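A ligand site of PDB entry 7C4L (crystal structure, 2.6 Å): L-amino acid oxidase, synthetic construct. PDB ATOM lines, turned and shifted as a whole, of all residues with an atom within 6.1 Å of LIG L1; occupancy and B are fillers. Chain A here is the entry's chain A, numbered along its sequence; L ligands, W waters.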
ATOM      1  N   GLY A  88      -7.085 -14.578  14.025  1.00  0.00           N
ATOM      2  CA  GLY A  88      -6.701 -13.420  13.241  1.00  0.00           C
ATOM      3  C   GLY A  88      -5.322 -13.435  12.634  1.00  0.00           C
ATOM      4  O   GLY A  88      -4.398 -13.953  13.262  1.00  0.00           O
ATOM      5  N   MET A  89      -5.166 -12.851  11.440  1.00  0.00           N
ATOM      6  CA  MET A  89      -3.938 -12.992  10.661  1.00  0.00           C
ATOM      7  C   MET A  89      -3.534 -11.786   9.818  1.00  0.00           C
ATOM      8  O   MET A  89      -2.358 -11.665   9.467  1.00  0.00           O
ATOM      9  CB  MET A  89      -4.036 -14.213   9.733  1.00  0.00           C
ATOM     10  CG  MET A  89      -4.870 -13.976   8.465  1.00  0.00           C
ATOM     11  SD  MET A  89      -4.929 -15.369   7.298  1.00  0.00           S
ATOM     12  CE  MET A  89      -3.522 -16.312   7.803  1.00  0.00           C
ATOM     13  N   ARG A  90      -4.467 -10.903   9.423  1.00  0.00           N
ATOM     14  CA  ARG A  90      -4.140  -9.850   8.460  1.00  0.00           C
ATOM     15  C   ARG A  90      -4.810  -8.544   8.850  1.00  0.00           C
ATOM     16  O   ARG A  90      -5.758  -8.531   9.648  1.00  0.00           O
ATOM     17  CB  ARG A  90      -4.555 -10.241   7.016  1.00  0.00           C
ATOM     18  CG  ARG A  90      -6.006 -10.759   6.863  1.00  0.00           C
ATOM     19  CD  ARG A  90      -6.362 -11.179   5.410  1.00  0.00           C
ATOM     20  NE  ARG A  90      -7.651 -11.877   5.292  1.00  0.00           N
ATOM     21  CZ  ARG A  90      -7.844 -13.011   4.598  1.00  0.00           C
ATOM     22  NH1 ARG A  90      -6.831 -13.591   3.950  1.00  0.00           N
ATOM     23  NH2 ARG A  90      -9.043 -13.570   4.569  1.00  0.00           N
ATOM     24  N   PHE A 232     -15.978 -18.701   1.504  1.00  0.00           N
ATOM     25  CA  PHE A 232     -16.626 -18.439   2.781  1.00  0.00           C
ATOM     26  C   PHE A 232     -18.124 -18.183   2.571  1.00  0.00           C
ATOM     27  O   PHE A 232     -18.610 -17.046   2.522  1.00  0.00           O
ATOM     28  CB  PHE A 232     -15.900 -17.329   3.485  1.00  0.00           C
ATOM     29  CG  PHE A 232     -14.485 -17.745   3.888  1.00  0.00           C
ATOM     30  CD1 PHE A 232     -13.404 -17.515   3.050  1.00  0.00           C
ATOM     31  CD2 PHE A 232     -14.261 -18.429   5.070  1.00  0.00           C
ATOM     32  CE1 PHE A 232     -12.114 -17.925   3.403  1.00  0.00           C
ATOM     33  CE2 PHE A 232     -12.974 -18.823   5.418  1.00  0.00           C
ATOM     34  CZ  PHE A 232     -11.909 -18.563   4.584  1.00  0.00           C
ATOM     35  N   LEU A 248     -18.070  -7.540   3.779  1.00  0.00           N
ATOM     36  CA  LEU A 248     -17.030  -8.569   3.839  1.00  0.00           C
ATOM     37  C   LEU A 248     -16.519  -8.954   2.452  1.00  0.00           C
ATOM     38  O   LEU A 248     -15.306  -9.164   2.283  1.00  0.00           O
ATOM     39  CB  LEU A 248     -17.580  -9.779   4.592  1.00  0.00           C
ATOM     40  CG  LEU A 248     -16.603 -10.868   5.026  1.00  0.00           C
ATOM     41  CD1 LEU A 248     -15.259 -10.289   5.475  1.00  0.00           C
ATOM     42  CD2 LEU A 248     -17.269 -11.689   6.117  1.00  0.00           C
ATOM     43  N   PHE A 252     -11.783  -7.745   0.063  1.00  0.00           N
ATOM     44  CA  PHE A 252     -10.683  -8.449  -0.580  1.00  0.00           C
ATOM     45  C   PHE A 252     -10.677  -8.152  -2.076  1.00  0.00           C
ATOM     46  O   PHE A 252     -10.992  -9.037  -2.890  1.00  0.00           O
ATOM     47  CB  PHE A 252     -10.779  -9.964  -0.359  1.00  0.00           C
ATOM     48  CG  PHE A 252     -10.966 -10.381   1.091  1.00  0.00           C
ATOM     49  CD1 PHE A 252      -9.874 -10.483   1.956  1.00  0.00           C
ATOM     50  CD2 PHE A 252     -12.231 -10.687   1.595  1.00  0.00           C
ATOM     51  CE1 PHE A 252     -10.030 -10.866   3.293  1.00  0.00           C
ATOM     52  CE2 PHE A 252     -12.408 -11.079   2.915  1.00  0.00           C
ATOM     53  CZ  PHE A 252     -11.299 -11.169   3.766  1.00  0.00           C
ATOM     54  N   LEU A 364     -16.235 -20.272  12.635  1.00  0.00           N
ATOM     55  CA  LEU A 364     -15.046 -20.323  11.809  1.00  0.00           C
ATOM     56  C   LEU A 364     -14.151 -21.441  12.322  1.00  0.00           C
ATOM     57  O   LEU A 364     -14.274 -21.879  13.472  1.00  0.00           O
ATOM     58  CB  LEU A 364     -14.253 -19.018  11.845  1.00  0.00           C
ATOM     59  CG  LEU A 364     -14.962 -17.743  11.377  1.00  0.00           C
ATOM     60  CD1 LEU A 364     -14.074 -16.500  11.434  1.00  0.00           C
ATOM     61  CD2 LEU A 364     -15.480 -17.951   9.977  1.00  0.00           C
ATOM     62  N   LYS A 366      -9.832 -23.032  11.891  1.00  0.00           N
ATOM     63  CA  LYS A 366      -8.506 -23.051  11.281  1.00  0.00           C
ATOM     64  C   LYS A 366      -7.771 -24.265  11.813  1.00  0.00           C
ATOM     65  O   LYS A 366      -7.598 -24.401  13.025  1.00  0.00           O
ATOM     66  CB  LYS A 366      -7.728 -21.775  11.581  1.00  0.00           C
ATOM     67  CG  LYS A 366      -8.082 -20.580  10.726  1.00  0.00           C
ATOM     68  CD  LYS A 366      -7.141 -19.405  10.998  1.00  0.00           C
ATOM     69  CE  LYS A 366      -7.463 -18.229  10.080  1.00  0.00           C
ATOM     70  NZ  LYS A 366      -6.371 -17.199  10.034  1.00  0.00           N
ATOM     71  N   TYR A 401      -4.293 -21.688   2.995  1.00  0.00           N
ATOM     72  CA  TYR A 401      -3.306 -20.612   2.959  1.00  0.00           C
ATOM     73  C   TYR A 401      -1.945 -21.143   3.380  1.00  0.00           C
ATOM     74  O   TYR A 401      -1.818 -21.766   4.451  1.00  0.00           O
ATOM     75  CB  TYR A 401      -3.691 -19.457   3.874  1.00  0.00           C
ATOM     76  CG  TYR A 401      -4.801 -18.533   3.415  1.00  0.00           C
ATOM     77  CD1 TYR A 401      -6.143 -18.860   3.640  1.00  0.00           C
ATOM     78  CD2 TYR A 401      -4.519 -17.294   2.843  1.00  0.00           C
ATOM     79  CE1 TYR A 401      -7.163 -18.004   3.248  1.00  0.00           C
ATOM     80  CE2 TYR A 401      -5.539 -16.438   2.451  1.00  0.00           C
ATOM     81  CZ  TYR A 401      -6.856 -16.791   2.658  1.00  0.00           C
ATOM     82  OH  TYR A 401      -7.852 -15.929   2.293  1.00  0.00           O
ATOM     83  N   TYR A 448      -8.914 -22.851   6.351  1.00  0.00           N
ATOM     84  CA  TYR A 448      -9.693 -21.752   6.919  1.00  0.00           C
ATOM     85  C   TYR A 448     -11.059 -21.809   6.243  1.00  0.00           C
ATOM     86  O   TYR A 448     -11.177 -21.532   5.045  1.00  0.00           O
ATOM     87  CB  TYR A 448      -8.940 -20.434   6.704  1.00  0.00           C
ATOM     88  CG  TYR A 448      -9.605 -19.183   7.221  1.00  0.00           C
ATOM     89  CD1 TYR A 448     -10.542 -19.238   8.239  1.00  0.00           C
ATOM     90  CD2 TYR A 448      -9.285 -17.924   6.674  1.00  0.00           C
ATOM     91  CE1 TYR A 448     -11.169 -18.095   8.694  1.00  0.00           C
ATOM     92  CE2 TYR A 448      -9.892 -16.773   7.124  1.00  0.00           C
ATOM     93  CZ  TYR A 448     -10.841 -16.872   8.144  1.00  0.00           C
ATOM     94  OH  TYR A 448     -11.478 -15.759   8.627  1.00  0.00           O
ATOM     95  N   ASP A 450     -15.709 -21.869   6.908  1.00  0.00           N
ATOM     96  CA  ASP A 450     -16.781 -21.201   7.640  1.00  0.00           C
ATOM     97  C   ASP A 450     -18.091 -21.954   7.413  1.00  0.00           C
ATOM     98  O   ASP A 450     -18.099 -23.050   6.838  1.00  0.00           O
ATOM     99  CB  ASP A 450     -16.916 -19.753   7.185  1.00  0.00           C
ATOM    100  CG  ASP A 450     -17.692 -19.642   5.887  1.00  0.00           C
ATOM    101  OD1 ASP A 450     -17.494 -20.494   4.997  1.00  0.00           O
ATOM    102  OD2 ASP A 450     -18.506 -18.706   5.766  1.00  0.00           O
ATOM    103  N   VAL A 536     -16.559 -15.073  14.405  1.00  0.00           N
ATOM    104  CA  VAL A 536     -16.898 -13.767  13.860  1.00  0.00           C
ATOM    105  C   VAL A 536     -18.395 -13.590  14.050  1.00  0.00           C
ATOM    106  O   VAL A 536     -19.101 -14.533  14.389  1.00  0.00           O
ATOM    107  CB  VAL A 536     -16.434 -13.670  12.378  1.00  0.00           C
ATOM    108  CG1 VAL A 536     -17.256 -12.694  11.500  1.00  0.00           C
ATOM    109  CG2 VAL A 536     -14.975 -13.293  12.338  1.00  0.00           C
ATOM    110  N   HIS A 537     -18.884 -12.358  13.887  1.00  0.00           N
ATOM    111  CA  HIS A 537     -20.312 -12.119  13.869  1.00  0.00           C
ATOM    112  C   HIS A 537     -20.663 -11.232  12.690  1.00  0.00           C
ATOM    113  O   HIS A 537     -19.800 -10.589  12.103  1.00  0.00           O
ATOM    114  CB  HIS A 537     -20.767 -11.473  15.172  1.00  0.00           C
ATOM    115  CG  HIS A 537     -20.331 -12.233  16.360  1.00  0.00           C
ATOM    116  ND1 HIS A 537     -19.014 -12.266  16.779  1.00  0.00           N
ATOM    117  CD2 HIS A 537     -21.011 -13.067  17.183  1.00  0.00           C
ATOM    118  CE1 HIS A 537     -18.916 -13.055  17.842  1.00  0.00           C
ATOM    119  NE2 HIS A 537     -20.113 -13.548  18.102  1.00  0.00           N
ATOM    120  N   GLN A 538     -21.935 -11.211  12.350  1.00  0.00           N
ATOM    121  CA  GLN A 538     -22.364 -10.328  11.289  1.00  0.00           C
ATOM    122  C   GLN A 538     -23.830 -10.000  11.493  1.00  0.00           C
ATOM    123  O   GLN A 538     -24.609 -10.840  11.939  1.00  0.00           O
ATOM    124  CB  GLN A 538     -22.137 -10.940   9.906  1.00  0.00           C
ATOM    125  CG  GLN A 538     -20.875 -10.474   9.219  1.00  0.00           C
ATOM    126  CD  GLN A 538     -19.721 -11.410   9.444  1.00  0.00           C
ATOM    127  OE1 GLN A 538     -19.869 -12.642   9.328  1.00  0.00           O
ATOM    128  NE2 GLN A 538     -18.558 -10.858   9.764  1.00  0.00           N
ATOM    129  N   GLN A 570     -17.489  -5.625  11.700  1.00  0.00           N
ATOM    130  CA  GLN A 570     -17.474  -6.999  12.146  1.00  0.00           C
ATOM    131  C   GLN A 570     -16.438  -7.827  11.387  1.00  0.00           C
ATOM    132  O   GLN A 570     -16.253  -7.674  10.166  1.00  0.00           O
ATOM    133  CB  GLN A 570     -18.865  -7.603  11.976  1.00  0.00           C
ATOM    134  CG  GLN A 570     -19.736  -7.368  13.174  1.00  0.00           C
ATOM    135  CD  GLN A 570     -21.194  -7.295  12.811  1.00  0.00           C
ATOM    136  OE1 GLN A 570     -21.536  -6.924  11.697  1.00  0.00           O
ATOM    137  NE2 GLN A 570     -22.049  -7.653  13.744  1.00  0.00           N
ATOM    138  N   GLY A 571     -15.726  -8.678  12.136  1.00  0.00           N
ATOM    139  CA  GLY A 571     -14.775  -9.623  11.574  1.00  0.00           C
ATOM    140  C   GLY A 571     -13.329  -9.213  11.671  1.00  0.00           C
ATOM    141  O   GLY A 571     -12.453  -9.971  11.232  1.00  0.00           O
ATOM    142  N   TRP A 572     -13.058  -8.036  12.237  1.00  0.00           N
ATOM    143  CA  TRP A 572     -11.747  -7.405  12.212  1.00  0.00           C
ATOM    144  C   TRP A 572     -11.461  -6.799  13.574  1.00  0.00           C
ATOM    145  O   TRP A 572     -12.377  -6.499  14.351  1.00  0.00           O
ATOM    146  CB  TRP A 572     -11.674  -6.325  11.121  1.00  0.00           C
ATOM    147  CG  TRP A 572     -11.908  -6.883   9.766  1.00  0.00           C
ATOM    148  CD1 TRP A 572     -13.102  -7.019   9.132  1.00  0.00           C
ATOM    149  CD2 TRP A 572     -10.916  -7.427   8.881  1.00  0.00           C
ATOM    150  NE1 TRP A 572     -12.917  -7.612   7.906  1.00  0.00           N
ATOM    151  CE2 TRP A 572     -11.588  -7.863   7.735  1.00  0.00           C
ATOM    152  CE3 TRP A 572      -9.534  -7.578   8.957  1.00  0.00           C
ATOM    153  CZ2 TRP A 572     -10.926  -8.447   6.662  1.00  0.00           C
ATOM    154  CZ3 TRP A 572      -8.868  -8.165   7.893  1.00  0.00           C
ATOM    155  CH2 TRP A 572      -9.563  -8.579   6.752  1.00  0.00           C
HETATM  156  N1  LIG L   1     -10.620 -10.729   8.988  1.00  0.00           N
HETATM  157  C1  LIG L   1     -11.178 -12.073   8.782  1.00  0.00           C
HETATM  158  C2  LIG L   1     -10.290 -12.933   7.857  1.00  0.00           C
HETATM  159  O1  LIG L   1      -9.069 -12.734   7.728  1.00  0.00           O
HETATM  160  C3  LIG L   1     -12.613 -11.989   8.235  1.00  0.00           C
HETATM  161  C4  LIG L   1     -13.500 -13.156   8.650  1.00  0.00           C
HETATM  162  C5  LIG L   1     -14.953 -12.948   8.329  1.00  0.00           C
HETATM  163  O2  LIG L   1     -15.555 -11.955   8.738  1.00  0.00           O
HETATM  164  N2  LIG L   1     -15.531 -13.897   7.586  1.00  0.00           N
HETATM  165  O3  LIG L   1     -10.740 -13.889   7.219  1.00  0.00           O
HETATM  166  P1  LG2 L   2     -12.441 -11.751  21.877  1.00  0.00           P
HETATM  167  O1  LG2 L   2     -11.061 -11.655  21.294  1.00  0.00           O
HETATM  168  O2  LG2 L   2     -13.085 -13.088  21.539  1.00  0.00           O
HETATM  169  O3  LG2 L   2     -12.481 -11.488  23.434  1.00  0.00           O
HETATM  170  C1  LG2 L   2     -13.367 -12.221  24.314  1.00  0.00           C
HETATM  171  C2  LG2 L   2     -12.579 -12.708  25.509  1.00  0.00           C
HETATM  172  O4  LG2 L   2     -13.422 -12.748  26.686  1.00  0.00           O
HETATM  173  C3  LG2 L   2     -11.952 -14.098  25.377  1.00  0.00           C
HETATM  174  O5  LG2 L   2     -10.641 -14.079  25.894  1.00  0.00           O
HETATM  175  C4  LG2 L   2     -12.838 -14.967  26.269  1.00  0.00           C
HETATM  176  O6  LG2 L   2     -12.083 -16.063  26.776  1.00  0.00           O
HETATM  177  C5  LG2 L   2     -13.190 -13.960  27.369  1.00  0.00           C
HETATM  178  N1  LG2 L   2     -14.382 -14.280  28.154  1.00  0.00           N
HETATM  179  C6  LG2 L   2     -15.579 -14.751  27.694  1.00  0.00           C
HETATM  180  N2  LG2 L   2     -16.479 -14.941  28.643  1.00  0.00           N
HETATM  181  C7  LG2 L   2     -15.828 -14.567  29.799  1.00  0.00           C
HETATM  182  C8  LG2 L   2     -16.221 -14.531  31.151  1.00  0.00           C
HETATM  183  N3  LG2 L   2     -17.430 -14.907  31.588  1.00  0.00           N
HETATM  184  N4  LG2 L   2     -15.318 -14.105  32.058  1.00  0.00           N
HETATM  185  C9  LG2 L   2     -14.109 -13.742  31.639  1.00  0.00           C
HETATM  186  N5  LG2 L   2     -13.612 -13.734  30.395  1.00  0.00           N
HETATM  187  C10 LG2 L   2     -14.528 -14.161  29.515  1.00  0.00           C
HETATM  188  N6  LG2 L   2      -9.535  -9.733  12.496  1.00  0.00           N
HETATM  189  C11 LG2 L   2      -8.722  -9.013  11.662  1.00  0.00           C
HETATM  190  O7  LG2 L   2      -8.621  -7.778  11.753  1.00  0.00           O
HETATM  191  N7  LG2 L   2      -7.969  -9.664  10.700  1.00  0.00           N
HETATM  192  C12 LG2 L   2      -7.951 -11.032  10.476  1.00  0.00           C
HETATM  193  O8  LG2 L   2      -7.244 -11.512   9.587  1.00  0.00           O
HETATM  194  C13 LG2 L   2      -8.820 -11.780  11.356  1.00  0.00           C
HETATM  195  N8  LG2 L   2      -8.868 -13.054  11.198  1.00  0.00           N
HETATM  196  C14 LG2 L   2      -9.687 -13.782  12.032  1.00  0.00           C
HETATM  197  C15 LG2 L   2      -9.721 -15.153  11.871  1.00  0.00           C
HETATM  198  C16 LG2 L   2     -10.516 -15.946  12.697  1.00  0.00           C
HETATM  199  C17 LG2 L   2     -10.538 -17.440  12.503  1.00  0.00           C
HETATM  200  C18 LG2 L   2     -11.290 -15.342  13.696  1.00  0.00           C
HETATM  201  C19 LG2 L   2     -12.139 -16.192  14.591  1.00  0.00           C
HETATM  202  C20 LG2 L   2     -11.256 -13.958  13.861  1.00  0.00           C
HETATM  203  C21 LG2 L   2     -10.454 -13.171  13.031  1.00  0.00           C
HETATM  204  N9  LG2 L   2     -10.377 -11.774  13.172  1.00  0.00           N
HETATM  205  C22 LG2 L   2      -9.574 -11.044  12.334  1.00  0.00           C
HETATM  206  C23 LG2 L   2     -11.187 -11.053  14.156  1.00  0.00           C
HETATM  207  C24 LG2 L   2     -10.490 -10.799  15.479  1.00  0.00           C
HETATM  208  O9  LG2 L   2      -9.942 -12.016  15.972  1.00  0.00           O
HETATM  209  C25 LG2 L   2     -11.527 -10.290  16.483  1.00  0.00           C
HETATM  210  O10 LG2 L   2     -12.277  -9.260  15.852  1.00  0.00           O
HETATM  211  C26 LG2 L   2     -11.021  -9.810  17.842  1.00  0.00           C
HETATM  212  O11 LG2 L   2      -9.795 -10.450  18.179  1.00  0.00           O
HETATM  213  C27 LG2 L   2     -12.055 -10.102  18.899  1.00  0.00           C
HETATM  214  O12 LG2 L   2     -12.015  -9.085  19.918  1.00  0.00           O
HETATM  215  P2  LG2 L   2     -13.023  -9.091  21.125  1.00  0.00           P
HETATM  216  O13 LG2 L   2     -12.256  -8.698  22.399  1.00  0.00           O
HETATM  217  O14 LG2 L   2     -14.231  -8.335  20.673  1.00  0.00           O
HETATM  218  O15 LG2 L   2     -13.374 -10.628  21.280  1.00  0.00           O
HETATM  219  O   HOH W   1      -7.717 -14.795   9.204  1.00  0.00           O
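Water W1 lies within hydrogen-bond range of O1 of LIG L1 (2.9 Å), NZ of Lys 366 (2.9 Å), N8 of LG2 L2 (2.9 Å) and SD of Met 89 (3.4 Å).
O8 of LG2 L2 sits close to O1 of LIG L1 (2.9 Å).
CD2 of Leu 248 touches O2 of LIG L1, 3.1 Å away.
Val 536 touches LIG L1.
Trp 572 touches LIG L1.
Of the 17 residues printed, 7 come within 4 Å of LIG L1.
The nearest printed residue that does not touch LIG L1 is Leu 364 (4.4 Å).
A nitrogen (N7) of LG2 L2 sits at hydrogen-bond distance from the backbone carbonyl oxygen (O) of Arg 90 (2.7 Å).
An oxygen (O2) of LIG L1 is in hydrogen-bond range of the side-chain amide nitrogen (NE2) of Gln 538.
The backbone NH of Met 89 is in hydrogen-bond range of an oxygen (O8) of LG2 L2, 3.1 Å away.
N of Arg 90 is in hydrogen-bond range of O8 of LG2 L2 (2.8 Å).
NE of Arg 90 is in salt-bridge range of O1 of LIG L1, at 2.9 Å.
The backbone carbonyl oxygen (O) of Trp 572 lies within hydrogen-bond range of an oxygen (O10) of LG2 L2 (3.1 Å).
O of Gly 571 is in hydrogen-bond range of N1 of LIG L1, at 3.0 Å.
The side-chain hydroxyl (OH) of Tyr 448 is in hydrogen-bond range of an oxygen (O3) of LIG L1 (2.5 Å).
NH1 of Arg 90 is in hydrogen-bond range of OH of Tyr 401 (3.0 Å).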
